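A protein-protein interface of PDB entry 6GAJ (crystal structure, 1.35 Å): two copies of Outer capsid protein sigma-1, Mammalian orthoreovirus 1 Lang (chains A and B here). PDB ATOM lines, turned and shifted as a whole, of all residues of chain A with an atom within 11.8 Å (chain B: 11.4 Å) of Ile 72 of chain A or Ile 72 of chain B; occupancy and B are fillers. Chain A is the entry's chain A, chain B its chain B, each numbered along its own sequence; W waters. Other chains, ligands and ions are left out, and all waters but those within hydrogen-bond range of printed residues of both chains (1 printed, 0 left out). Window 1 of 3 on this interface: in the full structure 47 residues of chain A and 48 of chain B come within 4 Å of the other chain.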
ATOM      1  N   LEU A  61      33.584 -34.661 -38.692  1.00  0.00           N
ATOM      2  CA  LEU A  61      32.815 -35.088 -37.546  1.00  0.00           C
ATOM      3  C   LEU A  61      33.265 -34.383 -36.291  1.00  0.00           C
ATOM      4  O   LEU A  61      32.404 -33.988 -35.464  1.00  0.00           O
ATOM      5  CB  LEU A  61      32.971 -36.584 -37.363  1.00  0.00           C
ATOM      6  CG  LEU A  61      31.827 -37.229 -36.598  1.00  0.00           C
ATOM      7  CD1 LEU A  61      30.460 -36.763 -37.120  1.00  0.00           C
ATOM      8  CD2 LEU A  61      31.914 -38.730 -36.622  1.00  0.00           C
ATOM      9  N   SER A  62      34.589 -34.148 -36.124  1.00  0.00           N
ATOM     10  CA  SER A  62      35.118 -33.462 -34.947  1.00  0.00           C
ATOM     11  C   SER A  62      34.542 -32.063 -34.883  1.00  0.00           C
ATOM     12  O   SER A  62      34.219 -31.567 -33.774  1.00  0.00           O
ATOM     13  CB  SER A  62      36.635 -33.381 -35.015  1.00  0.00           C
ATOM     14  OG  SER A  62      37.176 -34.686 -35.075  1.00  0.00           O
ATOM     15  N   ASN A  63      34.358 -31.414 -36.045  1.00  0.00           N
ATOM     16  CA  ASN A  63      33.821 -30.069 -36.059  1.00  0.00           C
ATOM     17  C   ASN A  63      32.316 -30.075 -35.670  1.00  0.00           C
ATOM     18  O   ASN A  63      31.869 -29.204 -34.897  1.00  0.00           O
ATOM     19  CB  ASN A  63      34.112 -29.410 -37.412  1.00  0.00           C
ATOM     20  CG  ASN A  63      35.606 -29.109 -37.637  1.00  0.00           C
ATOM     21  OD1 ASN A  63      36.428 -29.107 -36.712  1.00  0.00           O
ATOM     22  ND2 ASN A  63      35.995 -28.918 -38.907  1.00  0.00           N
ATOM     23  N   SER A  64      31.561 -31.096 -36.138  1.00  0.00           N
ATOM     24  CA  SER A  64      30.159 -31.254 -35.733  1.00  0.00           C
ATOM     25  C   SER A  64      30.074 -31.508 -34.204  1.00  0.00           C
ATOM     26  O   SER A  64      29.168 -30.982 -33.509  1.00  0.00           O
ATOM     27  CB  SER A  64      29.522 -32.432 -36.462  1.00  0.00           C
ATOM     28  OG  SER A  64      29.579 -32.242 -37.872  1.00  0.00           O
ATOM     29  N   VAL A  65      30.993 -32.351 -33.692  1.00  0.00           N
ATOM     30  CA  VAL A  65      31.031 -32.664 -32.245  1.00  0.00           C
ATOM     31  C   VAL A  65      31.335 -31.393 -31.482  1.00  0.00           C
ATOM     32  O   VAL A  65      30.678 -31.166 -30.472  1.00  0.00           O
ATOM     33  CB  VAL A  65      32.035 -33.791 -31.939  1.00  0.00           C
ATOM     34  CG1 VAL A  65      32.267 -33.999 -30.432  1.00  0.00           C
ATOM     35  CG2 VAL A  65      31.520 -35.088 -32.560  1.00  0.00           C
ATOM     36  N   SER A  66      32.269 -30.545 -31.971  1.00  0.00           N
ATOM     37  CA  SER A  66      32.608 -29.294 -31.299  1.00  0.00           C
ATOM     38  C   SER A  66      31.397 -28.388 -31.181  1.00  0.00           C
ATOM     39  O   SER A  66      31.157 -27.792 -30.083  1.00  0.00           O
ATOM     40  CB  SER A  66      33.722 -28.580 -32.053  1.00  0.00           C
ATOM     41  OG  SER A  66      33.843 -27.313 -31.437  1.00  0.00           O
ATOM     42  N   GLN A  67      30.591 -28.294 -32.225  1.00  0.00           N
ATOM     43  CA  GLN A  67      29.374 -27.504 -32.204  1.00  0.00           C
ATOM     44  C   GLN A  67      28.429 -28.061 -31.141  1.00  0.00           C
ATOM     45  O   GLN A  67      27.814 -27.300 -30.400  1.00  0.00           O
ATOM     46  CB  GLN A  67      28.693 -27.538 -33.553  1.00  0.00           C
ATOM     47  CG  GLN A  67      29.456 -26.770 -34.640  1.00  0.00           C
ATOM     48  CD  GLN A  67      29.384 -25.254 -34.514  1.00  0.00           C
ATOM     49  OE1 GLN A  67      28.438 -24.674 -33.951  1.00  0.00           O
ATOM     50  NE2 GLN A  67      30.403 -24.583 -35.033  1.00  0.00           N
ATOM     51  N   ASN A  68      28.321 -29.393 -31.053  1.00  0.00           N
ATOM     52  CA  ASN A  68      27.426 -29.998 -30.048  1.00  0.00           C
ATOM     53  C   ASN A  68      27.974 -29.813 -28.640  1.00  0.00           C
ATOM     54  O   ASN A  68      27.196 -29.526 -27.726  1.00  0.00           O
ATOM     55  CB  ASN A  68      27.229 -31.484 -30.327  1.00  0.00           C
ATOM     56  CG  ASN A  68      26.288 -31.729 -31.493  1.00  0.00           C
ATOM     57  OD1 ASN A  68      25.678 -30.808 -32.032  1.00  0.00           O
ATOM     58  ND2 ASN A  68      26.152 -32.980 -31.940  1.00  0.00           N
ATOM     59  N   THR A  69      29.295 -29.866 -28.447  1.00  0.00           N
ATOM     60  CA  THR A  69      29.831 -29.617 -27.110  1.00  0.00           C
ATOM     61  C   THR A  69      29.484 -28.184 -26.680  1.00  0.00           C
ATOM     62  O   THR A  69      29.099 -27.945 -25.531  1.00  0.00           O
ATOM     63  CB  THR A  69      31.342 -29.791 -27.157  1.00  0.00           C
ATOM     64  OG1 THR A  69      31.624 -31.116 -27.599  1.00  0.00           O
ATOM     65  CG2 THR A  69      32.003 -29.571 -25.801  1.00  0.00           C
ATOM     66  N   GLN A  70      29.546 -27.241 -27.639  1.00  0.00           N
ATOM     67  CA  GLN A  70      29.223 -25.821 -27.412  1.00  0.00           C
ATOM     68  C   GLN A  70      27.747 -25.671 -27.034  1.00  0.00           C
ATOM     69  O   GLN A  70      27.421 -24.928 -26.081  1.00  0.00           O
ATOM     70  CB  GLN A  70      29.589 -24.985 -28.656  1.00  0.00           C
ATOM     71  CG  GLN A  70      31.064 -24.623 -28.665  1.00  0.00           C
ATOM     72  CD  GLN A  70      31.532 -24.064 -29.965  1.00  0.00           C
ATOM     73  OE1 GLN A  70      32.543 -24.540 -30.511  1.00  0.00           O
ATOM     74  NE2 GLN A  70      30.813 -23.061 -30.473  1.00  0.00           N
ATOM     75  N   SER A  71      26.862 -26.355 -27.792  1.00  0.00           N
ATOM     76  CA  SER A  71      25.439 -26.287 -27.518  1.00  0.00           C
ATOM     77  C   SER A  71      25.136 -26.862 -26.151  1.00  0.00           C
ATOM     78  O   SER A  71      24.300 -26.312 -25.424  1.00  0.00           O
ATOM     79  CB  SER A  71      24.662 -27.096 -28.550  1.00  0.00           C
ATOM     80  OG  SER A  71      24.770 -26.531 -29.842  1.00  0.00           O
ATOM     81  N   ILE A  72      25.794 -27.941 -25.781  1.00  0.00           N
ATOM     82  CA  ILE A  72      25.600 -28.529 -24.467  1.00  0.00           C
ATOM     83  C   ILE A  72      26.021 -27.587 -23.376  1.00  0.00           C
ATOM     84  O   ILE A  72      25.312 -27.477 -22.351  1.00  0.00           O
ATOM     85  CB  ILE A  72      26.334 -29.875 -24.393  1.00  0.00           C
ATOM     86  CG1 ILE A  72      25.618 -30.917 -25.280  1.00  0.00           C
ATOM     87  CG2 ILE A  72      26.465 -30.350 -22.924  1.00  0.00           C
ATOM     88  CD1 ILE A  72      26.529 -32.141 -25.609  1.00  0.00           C
ATOM     89  N   SER A  73      27.128 -26.855 -23.569  1.00  0.00           N
ATOM     90  CA  SER A  73      27.583 -25.912 -22.556  1.00  0.00           C
ATOM     91  C   SER A  73      26.535 -24.799 -22.401  1.00  0.00           C
ATOM     92  O   SER A  73      26.224 -24.384 -21.268  1.00  0.00           O
ATOM     93  CB  SER A  73      28.922 -25.332 -23.009  1.00  0.00           C
ATOM     94  OG  SER A  73      29.471 -24.595 -21.934  1.00  0.00           O
ATOM     95  N   SER A  74      25.958 -24.316 -23.512  1.00  0.00           N
ATOM     96  CA  SER A  74      24.964 -23.262 -23.496  1.00  0.00           C
ATOM     97  C   SER A  74      23.725 -23.717 -22.726  1.00  0.00           C
ATOM     98  O   SER A  74      23.193 -22.983 -21.878  1.00  0.00           O
ATOM     99  CB  SER A  74      24.625 -22.813 -24.911  1.00  0.00           C
ATOM    100  OG  SER A  74      23.513 -21.924 -24.901  1.00  0.00           O
ATOM    101  N   LEU A  75      23.246 -24.955 -23.037  1.00  0.00           N
ATOM    102  CA  LEU A  75      22.061 -25.492 -22.367  1.00  0.00           C
ATOM    103  C   LEU A  75      22.356 -25.643 -20.870  1.00  0.00           C
ATOM    104  O   LEU A  75      21.476 -25.330 -20.036  1.00  0.00           O
ATOM    105  CB  LEU A  75      21.730 -26.818 -22.953  1.00  0.00           C
ATOM    106  CG  LEU A  75      21.183 -26.796 -24.377  1.00  0.00           C
ATOM    107  CD1 LEU A  75      20.960 -28.250 -24.869  1.00  0.00           C
ATOM    108  CD2 LEU A  75      19.842 -25.965 -24.472  1.00  0.00           C
ATOM    109  N   GLY A  76      23.562 -26.096 -20.514  1.00  0.00           N
ATOM    110  CA  GLY A  76      23.949 -26.240 -19.127  1.00  0.00           C
ATOM    111  C   GLY A  76      23.928 -24.911 -18.400  1.00  0.00           C
ATOM    112  O   GLY A  76      23.415 -24.823 -17.265  1.00  0.00           O
ATOM    113  N   ASP A  77      24.327 -23.829 -19.079  1.00  0.00           N
ATOM    114  CA  ASP A  77      24.314 -22.515 -18.424  1.00  0.00           C
ATOM    115  C   ASP A  77      22.860 -22.124 -18.156  1.00  0.00           C
ATOM    116  O   ASP A  77      22.514 -21.579 -17.110  1.00  0.00           O
ATOM    117  CB  ASP A  77      24.999 -21.491 -19.330  1.00  0.00           C
ATOM    118  CG  ASP A  77      26.546 -21.595 -19.306  1.00  0.00           C
ATOM    119  OD1 ASP A  77      27.090 -22.236 -18.378  1.00  0.00           O
ATOM    120  OD2 ASP A  77      27.188 -21.084 -20.256  1.00  0.00           O
ATOM    121  N   ARG A  78      21.975 -22.419 -19.123  1.00  0.00           N
ATOM    122  CA  ARG A  78      20.556 -22.048 -18.965  1.00  0.00           C
ATOM    123  C   ARG A  78      19.885 -22.861 -17.851  1.00  0.00           C
ATOM    124  O   ARG A  78      19.143 -22.267 -17.063  1.00  0.00           O
ATOM    125  CB  ARG A  78      19.816 -22.181 -20.281  1.00  0.00           C
ATOM    126  CG  ARG A  78      20.293 -21.108 -21.279  1.00  0.00           C
ATOM    127  CD  ARG A  78      19.824 -21.401 -22.687  1.00  0.00           C
ATOM    128  NE  ARG A  78      18.403 -21.113 -22.831  1.00  0.00           N
ATOM    129  CZ  ARG A  78      17.738 -21.379 -23.940  1.00  0.00           C
ATOM    130  NH1 ARG A  78      18.347 -22.000 -24.957  1.00  0.00           N
ATOM    131  NH2 ARG A  78      16.462 -21.040 -24.049  1.00  0.00           N
ATOM    132  N   ILE A  79      20.130 -24.170 -17.760  1.00  0.00           N
ATOM    133  CA  ILE A  79      19.510 -24.929 -16.668  1.00  0.00           C
ATOM    134  C   ILE A  79      20.132 -24.569 -15.310  1.00  0.00           C
ATOM    135  O   ILE A  79      19.409 -24.452 -14.307  1.00  0.00           O
ATOM    136  CB  ILE A  79      19.436 -26.441 -16.984  1.00  0.00           C
ATOM    137  CG1 ILE A  79      18.477 -27.166 -16.028  1.00  0.00           C
ATOM    138  CG2 ILE A  79      20.814 -27.105 -17.095  1.00  0.00           C
ATOM    139  CD1 ILE A  79      17.031 -26.955 -16.308  1.00  0.00           C
ATOM    140  N   ASN A  80      21.449 -24.244 -15.294  1.00  0.00           N
ATOM    141  CA  ASN A  80      22.091 -23.807 -14.023  1.00  0.00           C
ATOM    142  C   ASN A  80      21.438 -22.507 -13.534  1.00  0.00           C
ATOM    143  O   ASN A  80      21.324 -22.297 -12.328  1.00  0.00           O
ATOM    144  CB  ASN A  80      23.576 -23.453 -14.208  1.00  0.00           C
ATOM    145  CG  ASN A  80      24.519 -24.610 -14.371  1.00  0.00           C
ATOM    146  OD1 ASN A  80      24.178 -25.771 -14.113  1.00  0.00           O
ATOM    147  ND2 ASN A  80      25.739 -24.306 -14.835  1.00  0.00           N
ATOM    148  N   ALA A  81      20.993 -21.652 -14.460  1.00  0.00           N
ATOM    149  CA  ALA A  81      20.365 -20.402 -14.070  1.00  0.00           C
ATOM    150  C   ALA A  81      18.904 -20.581 -13.664  1.00  0.00           C
ATOM    151  O   ALA A  81      18.448 -19.901 -12.733  1.00  0.00           O
ATOM    152  CB  ALA A  81      20.481 -19.370 -15.201  1.00  0.00           C
ATOM    153  N   ASN B  63      26.520 -41.757 -36.739  1.00  0.00           N
ATOM    154  CA  ASN B  63      25.118 -41.964 -36.336  1.00  0.00           C
ATOM    155  C   ASN B  63      24.866 -41.423 -34.935  1.00  0.00           C
ATOM    156  O   ASN B  63      23.832 -40.784 -34.680  1.00  0.00           O
ATOM    157  CB  ASN B  63      24.769 -43.447 -36.406  1.00  0.00           C
ATOM    158  CG  ASN B  63      24.619 -43.946 -37.819  1.00  0.00           C
ATOM    159  OD1 ASN B  63      24.378 -43.179 -38.758  1.00  0.00           O
ATOM    160  ND2 ASN B  63      24.739 -45.259 -38.007  1.00  0.00           N
ATOM    161  N   SER B  64      25.776 -41.677 -34.002  1.00  0.00           N
ATOM    162  CA  SER B  64      25.655 -41.169 -32.658  1.00  0.00           C
ATOM    163  C   SER B  64      25.674 -39.665 -32.629  1.00  0.00           C
ATOM    164  O   SER B  64      24.864 -39.051 -31.888  1.00  0.00           O
ATOM    165  CB  SER B  64      26.815 -41.671 -31.787  1.00  0.00           C
ATOM    166  OG  SER B  64      26.736 -43.057 -31.610  1.00  0.00           O
ATOM    167  N   VAL B  65      26.531 -39.026 -33.439  1.00  0.00           N
ATOM    168  CA  VAL B  65      26.553 -37.552 -33.466  1.00  0.00           C
ATOM    169  C   VAL B  65      25.221 -37.041 -33.996  1.00  0.00           C
ATOM    170  O   VAL B  65      24.687 -36.064 -33.434  1.00  0.00           O
ATOM    171  CB  VAL B  65      27.730 -37.074 -34.338  1.00  0.00           C
ATOM    172  CG1 VAL B  65      27.674 -35.545 -34.580  1.00  0.00           C
ATOM    173  CG2 VAL B  65      29.059 -37.421 -33.660  1.00  0.00           C
ATOM    174  N   SER B  66      24.656 -37.651 -35.042  1.00  0.00           N
ATOM    175  CA  SER B  66      23.366 -37.187 -35.559  1.00  0.00           C
ATOM    176  C   SER B  66      22.246 -37.333 -34.508  1.00  0.00           C
ATOM    177  O   SER B  66      21.417 -36.417 -34.301  1.00  0.00           O
ATOM    178  CB  SER B  66      23.031 -38.021 -36.786  1.00  0.00           C
ATOM    179  OG  SER B  66      21.723 -37.748 -37.241  1.00  0.00           O
ATOM    180  N   GLN B  67      22.267 -38.418 -33.748  1.00  0.00           N
ATOM    181  CA  GLN B  67      21.255 -38.574 -32.714  1.00  0.00           C
ATOM    182  C   GLN B  67      21.445 -37.490 -31.661  1.00  0.00           C
ATOM    183  O   GLN B  67      20.469 -36.936 -31.152  1.00  0.00           O
ATOM    184  CB  GLN B  67      21.443 -39.930 -32.011  1.00  0.00           C
ATOM    185  CG  GLN B  67      21.060 -41.120 -32.847  1.00  0.00           C
ATOM    186  CD  GLN B  67      21.470 -42.418 -32.148  1.00  0.00           C
ATOM    187  OE1 GLN B  67      22.458 -42.535 -31.394  1.00  0.00           O
ATOM    188  NE2 GLN B  67      20.677 -43.443 -32.361  1.00  0.00           N
ATOM    189  N   ASN B  68      22.686 -37.208 -31.293  1.00  0.00           N
ATOM    190  CA  ASN B  68      22.941 -36.225 -30.232  1.00  0.00           C
ATOM    191  C   ASN B  68      22.605 -34.831 -30.725  1.00  0.00           C
ATOM    192  O   ASN B  68      22.072 -34.032 -29.950  1.00  0.00           O
ATOM    193  CB  ASN B  68      24.369 -36.290 -29.773  1.00  0.00           C
ATOM    194  CG  ASN B  68      24.656 -37.522 -28.920  1.00  0.00           C
ATOM    195  OD1 ASN B  68      23.760 -38.332 -28.633  1.00  0.00           O
ATOM    196  ND2 ASN B  68      25.924 -37.665 -28.506  1.00  0.00           N
ATOM    197  N   THR B  69      22.826 -34.523 -32.013  1.00  0.00           N
ATOM    198  CA  THR B  69      22.459 -33.181 -32.491  1.00  0.00           C
ATOM    199  C   THR B  69      20.941 -32.994 -32.305  1.00  0.00           C
ATOM    200  O   THR B  69      20.432 -31.941 -31.879  1.00  0.00           O
ATOM    201  CB  THR B  69      22.807 -33.117 -33.973  1.00  0.00           C
ATOM    202  OG1 THR B  69      24.219 -33.264 -34.107  1.00  0.00           O
ATOM    203  CG2 THR B  69      22.354 -31.752 -34.618  1.00  0.00           C
ATOM    204  N   GLN B  70      20.179 -34.056 -32.615  1.00  0.00           N
ATOM    205  CA  GLN B  70      18.718 -34.001 -32.482  1.00  0.00           C
ATOM    206  C   GLN B  70      18.295 -33.914 -31.014  1.00  0.00           C
ATOM    207  O   GLN B  70      17.376 -33.118 -30.667  1.00  0.00           O
ATOM    208  CB  GLN B  70      18.113 -35.236 -33.142  1.00  0.00           C
ATOM    209  CG  GLN B  70      16.620 -35.004 -33.317  1.00  0.00           C
ATOM    210  CD  GLN B  70      15.931 -36.152 -33.992  1.00  0.00           C
ATOM    211  OE1 GLN B  70      16.250 -36.480 -35.157  1.00  0.00           O
ATOM    212  NE2 GLN B  70      14.870 -36.662 -33.319  1.00  0.00           N
ATOM    213  N   SER B  71      18.902 -34.715 -30.133  1.00  0.00           N
ATOM    214  CA  SER B  71      18.572 -34.641 -28.714  1.00  0.00           C
ATOM    215  C   SER B  71      18.871 -33.250 -28.153  1.00  0.00           C
ATOM    216  O   SER B  71      18.127 -32.754 -27.309  1.00  0.00           O
ATOM    217  CB  SER B  71      19.400 -35.623 -27.907  1.00  0.00           C
ATOM    218  OG  SER B  71      19.048 -36.935 -28.327  1.00  0.00           O
ATOM    219  N   ILE B  72      19.981 -32.655 -28.584  1.00  0.00           N
ATOM    220  CA  ILE B  72      20.290 -31.285 -28.094  1.00  0.00           C
ATOM    221  C   ILE B  72      19.216 -30.332 -28.560  1.00  0.00           C
ATOM    222  O   ILE B  72      18.810 -29.455 -27.756  1.00  0.00           O
ATOM    223  CB  ILE B  72      21.667 -30.911 -28.658  1.00  0.00           C
ATOM    224  CG1 ILE B  72      22.754 -31.706 -27.886  1.00  0.00           C
ATOM    225  CG2 ILE B  72      21.933 -29.404 -28.550  1.00  0.00           C
ATOM    226  CD1 ILE B  72      24.136 -31.750 -28.551  1.00  0.00           C
ATOM    227  N   SER B  73      18.690 -30.489 -29.783  1.00  0.00           N
ATOM    228  CA  SER B  73      17.661 -29.566 -30.290  1.00  0.00           C
ATOM    229  C   SER B  73      16.386 -29.763 -29.430  1.00  0.00           C
ATOM    230  O   SER B  73      15.767 -28.756 -29.063  1.00  0.00           O
ATOM    231  CB  SER B  73      17.363 -29.968 -31.729  1.00  0.00           C
ATOM    232  OG  SER B  73      16.447 -29.003 -32.242  1.00  0.00           O
ATOM    233  N   SER B  74      16.025 -30.988 -29.072  1.00  0.00           N
ATOM    234  CA  SER B  74      14.842 -31.280 -28.258  1.00  0.00           C
ATOM    235  C   SER B  74      14.997 -30.643 -26.874  1.00  0.00           C
ATOM    236  O   SER B  74      14.046 -30.043 -26.346  1.00  0.00           O
ATOM    237  CB  SER B  74      14.676 -32.784 -28.079  1.00  0.00           C
ATOM    238  OG  SER B  74      13.617 -33.058 -27.169  1.00  0.00           O
ATOM    239  N   LEU B  75      16.185 -30.795 -26.260  1.00  0.00           N
ATOM    240  CA  LEU B  75      16.382 -30.191 -24.932  1.00  0.00           C
ATOM    241  C   LEU B  75      16.255 -28.661 -25.052  1.00  0.00           C
ATOM    242  O   LEU B  75      15.680 -28.029 -24.135  1.00  0.00           O
ATOM    243  CB  LEU B  75      17.810 -30.539 -24.413  1.00  0.00           C
ATOM    244  CG  LEU B  75      17.945 -32.018 -24.069  1.00  0.00           C
ATOM    245  CD1 LEU B  75      19.407 -32.321 -23.709  1.00  0.00           C
ATOM    246  CD2 LEU B  75      16.957 -32.437 -22.908  1.00  0.00           C
ATOM    247  N   GLY B  76      16.798 -28.095 -26.122  1.00  0.00           N
ATOM    248  CA  GLY B  76      16.683 -26.666 -26.332  1.00  0.00           C
ATOM    249  C   GLY B  76      15.244 -26.225 -26.454  1.00  0.00           C
ATOM    250  O   GLY B  76      14.866 -25.197 -25.869  1.00  0.00           O
ATOM    251  N   ASP B  77      14.391 -27.008 -27.097  1.00  0.00           N
ATOM    252  CA  ASP B  77      12.970 -26.606 -27.192  1.00  0.00           C
ATOM    253  C   ASP B  77      12.335 -26.649 -25.807  1.00  0.00           C
ATOM    254  O   ASP B  77      11.511 -25.773 -25.468  1.00  0.00           O
ATOM    255  CB  ASP B  77      12.201 -27.518 -28.162  1.00  0.00           C
ATOM    256  CG  ASP B  77      12.593 -27.366 -29.617  1.00  0.00           C
ATOM    257  OD1 ASP B  77      13.147 -26.312 -29.972  1.00  0.00           O
ATOM    258  OD2 ASP B  77      12.333 -28.306 -30.403  1.00  0.00           O
ATOM    259  N   ARG B  78      12.716 -27.619 -24.980  1.00  0.00           N
ATOM    260  CA  ARG B  78      12.159 -27.687 -23.626  1.00  0.00           C
ATOM    261  C   ARG B  78      12.637 -26.560 -22.720  1.00  0.00           C
ATOM    262  O   ARG B  78      11.823 -26.018 -21.961  1.00  0.00           O
ATOM    263  CB  ARG B  78      12.454 -29.049 -23.012  1.00  0.00           C
ATOM    264  CG  ARG B  78      11.617 -30.138 -23.713  1.00  0.00           C
ATOM    265  CD  ARG B  78      12.033 -31.540 -23.392  1.00  0.00           C
ATOM    266  NE  ARG B  78      11.736 -31.849 -21.971  1.00  0.00           N
ATOM    267  CZ  ARG B  78      12.269 -32.873 -21.318  1.00  0.00           C
ATOM    268  NH1 ARG B  78      13.157 -33.672 -21.928  1.00  0.00           N
ATOM    269  NH2 ARG B  78      11.913 -33.124 -20.053  1.00  0.00           N
ATOM    270  N   ILE B  79      13.930 -26.170 -22.783  1.00  0.00           N
ATOM    271  CA  ILE B  79      14.359 -25.092 -21.923  1.00  0.00           C
ATOM    272  C   ILE B  79      13.822 -23.780 -22.455  1.00  0.00           C
ATOM    273  O   ILE B  79      13.420 -22.942 -21.619  1.00  0.00           O
ATOM    274  CB  ILE B  79      15.890 -25.118 -21.656  1.00  0.00           C
ATOM    275  CG1 ILE B  79      16.304 -24.107 -20.557  1.00  0.00           C
ATOM    276  CG2 ILE B  79      16.692 -24.890 -22.949  1.00  0.00           C
ATOM    277  CD1 ILE B  79      15.949 -24.496 -19.172  1.00  0.00           C
ATOM    278  N   ASN B  80      13.702 -23.619 -23.790  1.00  0.00           N
ATOM    279  CA  ASN B  80      13.049 -22.436 -24.388  1.00  0.00           C
ATOM    280  C   ASN B  80      11.672 -22.236 -23.836  1.00  0.00           C
ATOM    281  O   ASN B  80      11.224 -21.083 -23.618  1.00  0.00           O
ATOM    282  CB  ASN B  80      12.846 -22.707 -25.875  1.00  0.00           C
ATOM    283  CG  ASN B  80      14.044 -22.386 -26.710  1.00  0.00           C
ATOM    284  OD1 ASN B  80      15.065 -21.932 -26.201  1.00  0.00           O
ATOM    285  ND2 ASN B  80      13.928 -22.609 -28.029  1.00  0.00           N
ATOM    286  N   ALA B  81      10.956 -23.329 -23.643  1.00  0.00           N
ATOM    287  CA  ALA B  81       9.572 -23.282 -23.166  1.00  0.00           C
ATOM    288  C   ALA B  81       9.482 -23.004 -21.660  1.00  0.00           C
ATOM    289  O   ALA B  81       8.558 -22.288 -21.189  1.00  0.00           O
ATOM    290  CB  ALA B  81       8.857 -24.573 -23.509  1.00  0.00           C
ATOM    291  N   GLU B  83      11.696 -21.338 -19.664  1.00  0.00           N
ATOM    292  CA  GLU B  83      12.155 -20.020 -19.232  1.00  0.00           C
ATOM    293  C   GLU B  83      11.032 -18.986 -19.097  1.00  0.00           C
ATOM    294  O   GLU B  83      10.899 -18.371 -18.044  1.00  0.00           O
ATOM    295  CB  GLU B  83      13.306 -19.553 -20.103  1.00  0.00           C
ATOM    296  CG  GLU B  83      14.629 -20.273 -19.813  1.00  0.00           C
ATOM    297  CD  GLU B  83      15.710 -19.942 -20.827  1.00  0.00           C
ATOM    298  OE1 GLU B  83      15.396 -19.409 -21.928  1.00  0.00           O
ATOM    299  OE2 GLU B  83      16.874 -20.258 -20.523  1.00  0.00           O
HETATM  300  O   HOH W   1      18.025 -19.885 -18.063  1.00  0.00           O
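The guanidinium group (NH2) of Arg 78 of chain A lies within salt-bridge range of the side-chain carboxylate (OE1) of Glu 83 of chain B (2.9 Å). NH2 of Arg 78 of chain A lies within hydrogen-bond range of OD1 of Asn 80 of chain B (2.7 Å). ND2 of Asn 68 of chain A is in hydrogen-bond range of OG1 of Thr 69 of chain B.
OG1 of Thr 69 of chain B is in hydrogen-bond range of O of Val 65 of chain B (2.9 Å). The backbone carbonyl oxygen (O) of Val 65 of chain A lies within hydrogen-bond range of the side-chain hydroxyl (OG1) of Thr 69 of chain A (3.0 Å). O of Gln 67 of chain A is in hydrogen-bond range of OG of Ser 71 of chain A (3.2 Å). OD1 of Asn 80 of chain B sits close to O of Gly 76 of chain B.
Val 65 of chain B touches Leu 61 of chain A (CG2 to CD1, 3.8 Å). CG2 of Val 65 of chain B touches CG2 of Val 65 of chain A, at 3.6 Å. Ser 71 of chain A touches Ile 72 of chain B. Ile 72 of chain A touches Ile 72 of chain B. CD1 of Leu 75 of chain A touches O of Ile 72 of chain B (3.8 Å). Leu 75 of chain B touches Leu 75 of chain A (CB to CD1, 3.9 Å). CA of Gly 76 of chain B touches CD2 of Leu 75 of chain A, at 3.7 Å. CD2 of Leu 75 of chain A touches CG2 of Ile 79 of chain B (3.7 Å). CG2 of Ile 79 of chain B touches CZ of Arg 78 of chain A (3.8 Å). CD1 of Ile 79 of chain A touches CD1 of Ile 79 of chain B, at 3.9 Å.
Of the printed residues of chain B, Leu 61 of chain A touches Val 65 (3.8 Å). Ser 64 of chain A touches none of the printed residues of chain B. Asn 68 of chain A touches just these residues of chain B: Val 65 (3.7 Å), Thr 69 (2.9 Å) and Ile 72 (3.6 Å). Thr 69 of chain A touches none of the printed residues of chain B. Ile 72 of chain A touches just one residue of chain B: Ile 72 (3.7 Å). No residue of chain B comes within 4 Å of Ser 74 of chain A. Printed residues of chain B within 4 Å of Leu 75 of chain A: Ile 72 (3.8 Å), Leu 75 (3.9 Å), Gly 76 (3.7 Å) and Ile 79 (3.7 Å). Gly 76 of chain A touches none of the printed residues of chain B. Of the printed residues of chain B, Arg 78 of chain A touches Ile 79, Asn 80 and Glu 83. Of the printed residues of chain B, Ile 79 of chain A touches Ile 79. Of chain A, only Asn 68 (2.9 Å) comes within 4 Å of Thr 69 of chain B. Of chain A, only Asn 68, Ser 71, Ile 72 and Leu 75 come within 4 Å of Ile 72 of chain B. Ser 73 of chain B touches none of the printed residues of chain A. Of the printed residues of chain A, Glu 83 of chain B touches Arg 78 (2.9 Å).
Hydrophobic or aromatic side chains of chain A that line the printed part of chain B: Leu 61, Val 65, Ile 72, Leu 75 and Ile 79. Along chain B the printed residues that touch a printed residue of chain A span positions 65 to 83.
Val 65 of chain A touches its own counterpart, Val 65 of chain B. Leu 75 of chain A touches Ile 72 of chain B, but with the chains exchanged Ile 72 of chain A does not touch Leu 75 of chain B (6.6 Å). Leu 75 of chain B touches its own counterpart, Leu 75 of chain A. Arg 78 of chain A touches Ile 79 of chain B, but with the chains exchanged Ile 79 of chain A does not touch Arg 78 of chain B (7.7 Å). 19 positions are printed for both chains. Of the 15 pairs that touch across the chains among the printed residues, 4 have their exchanged pair printed and touching as well.
Water W1 bridges the side-chain carboxylate (OE2) of Glu 83 of chain B and the backbone carbonyl oxygen (O) of Arg 78 of chain A.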
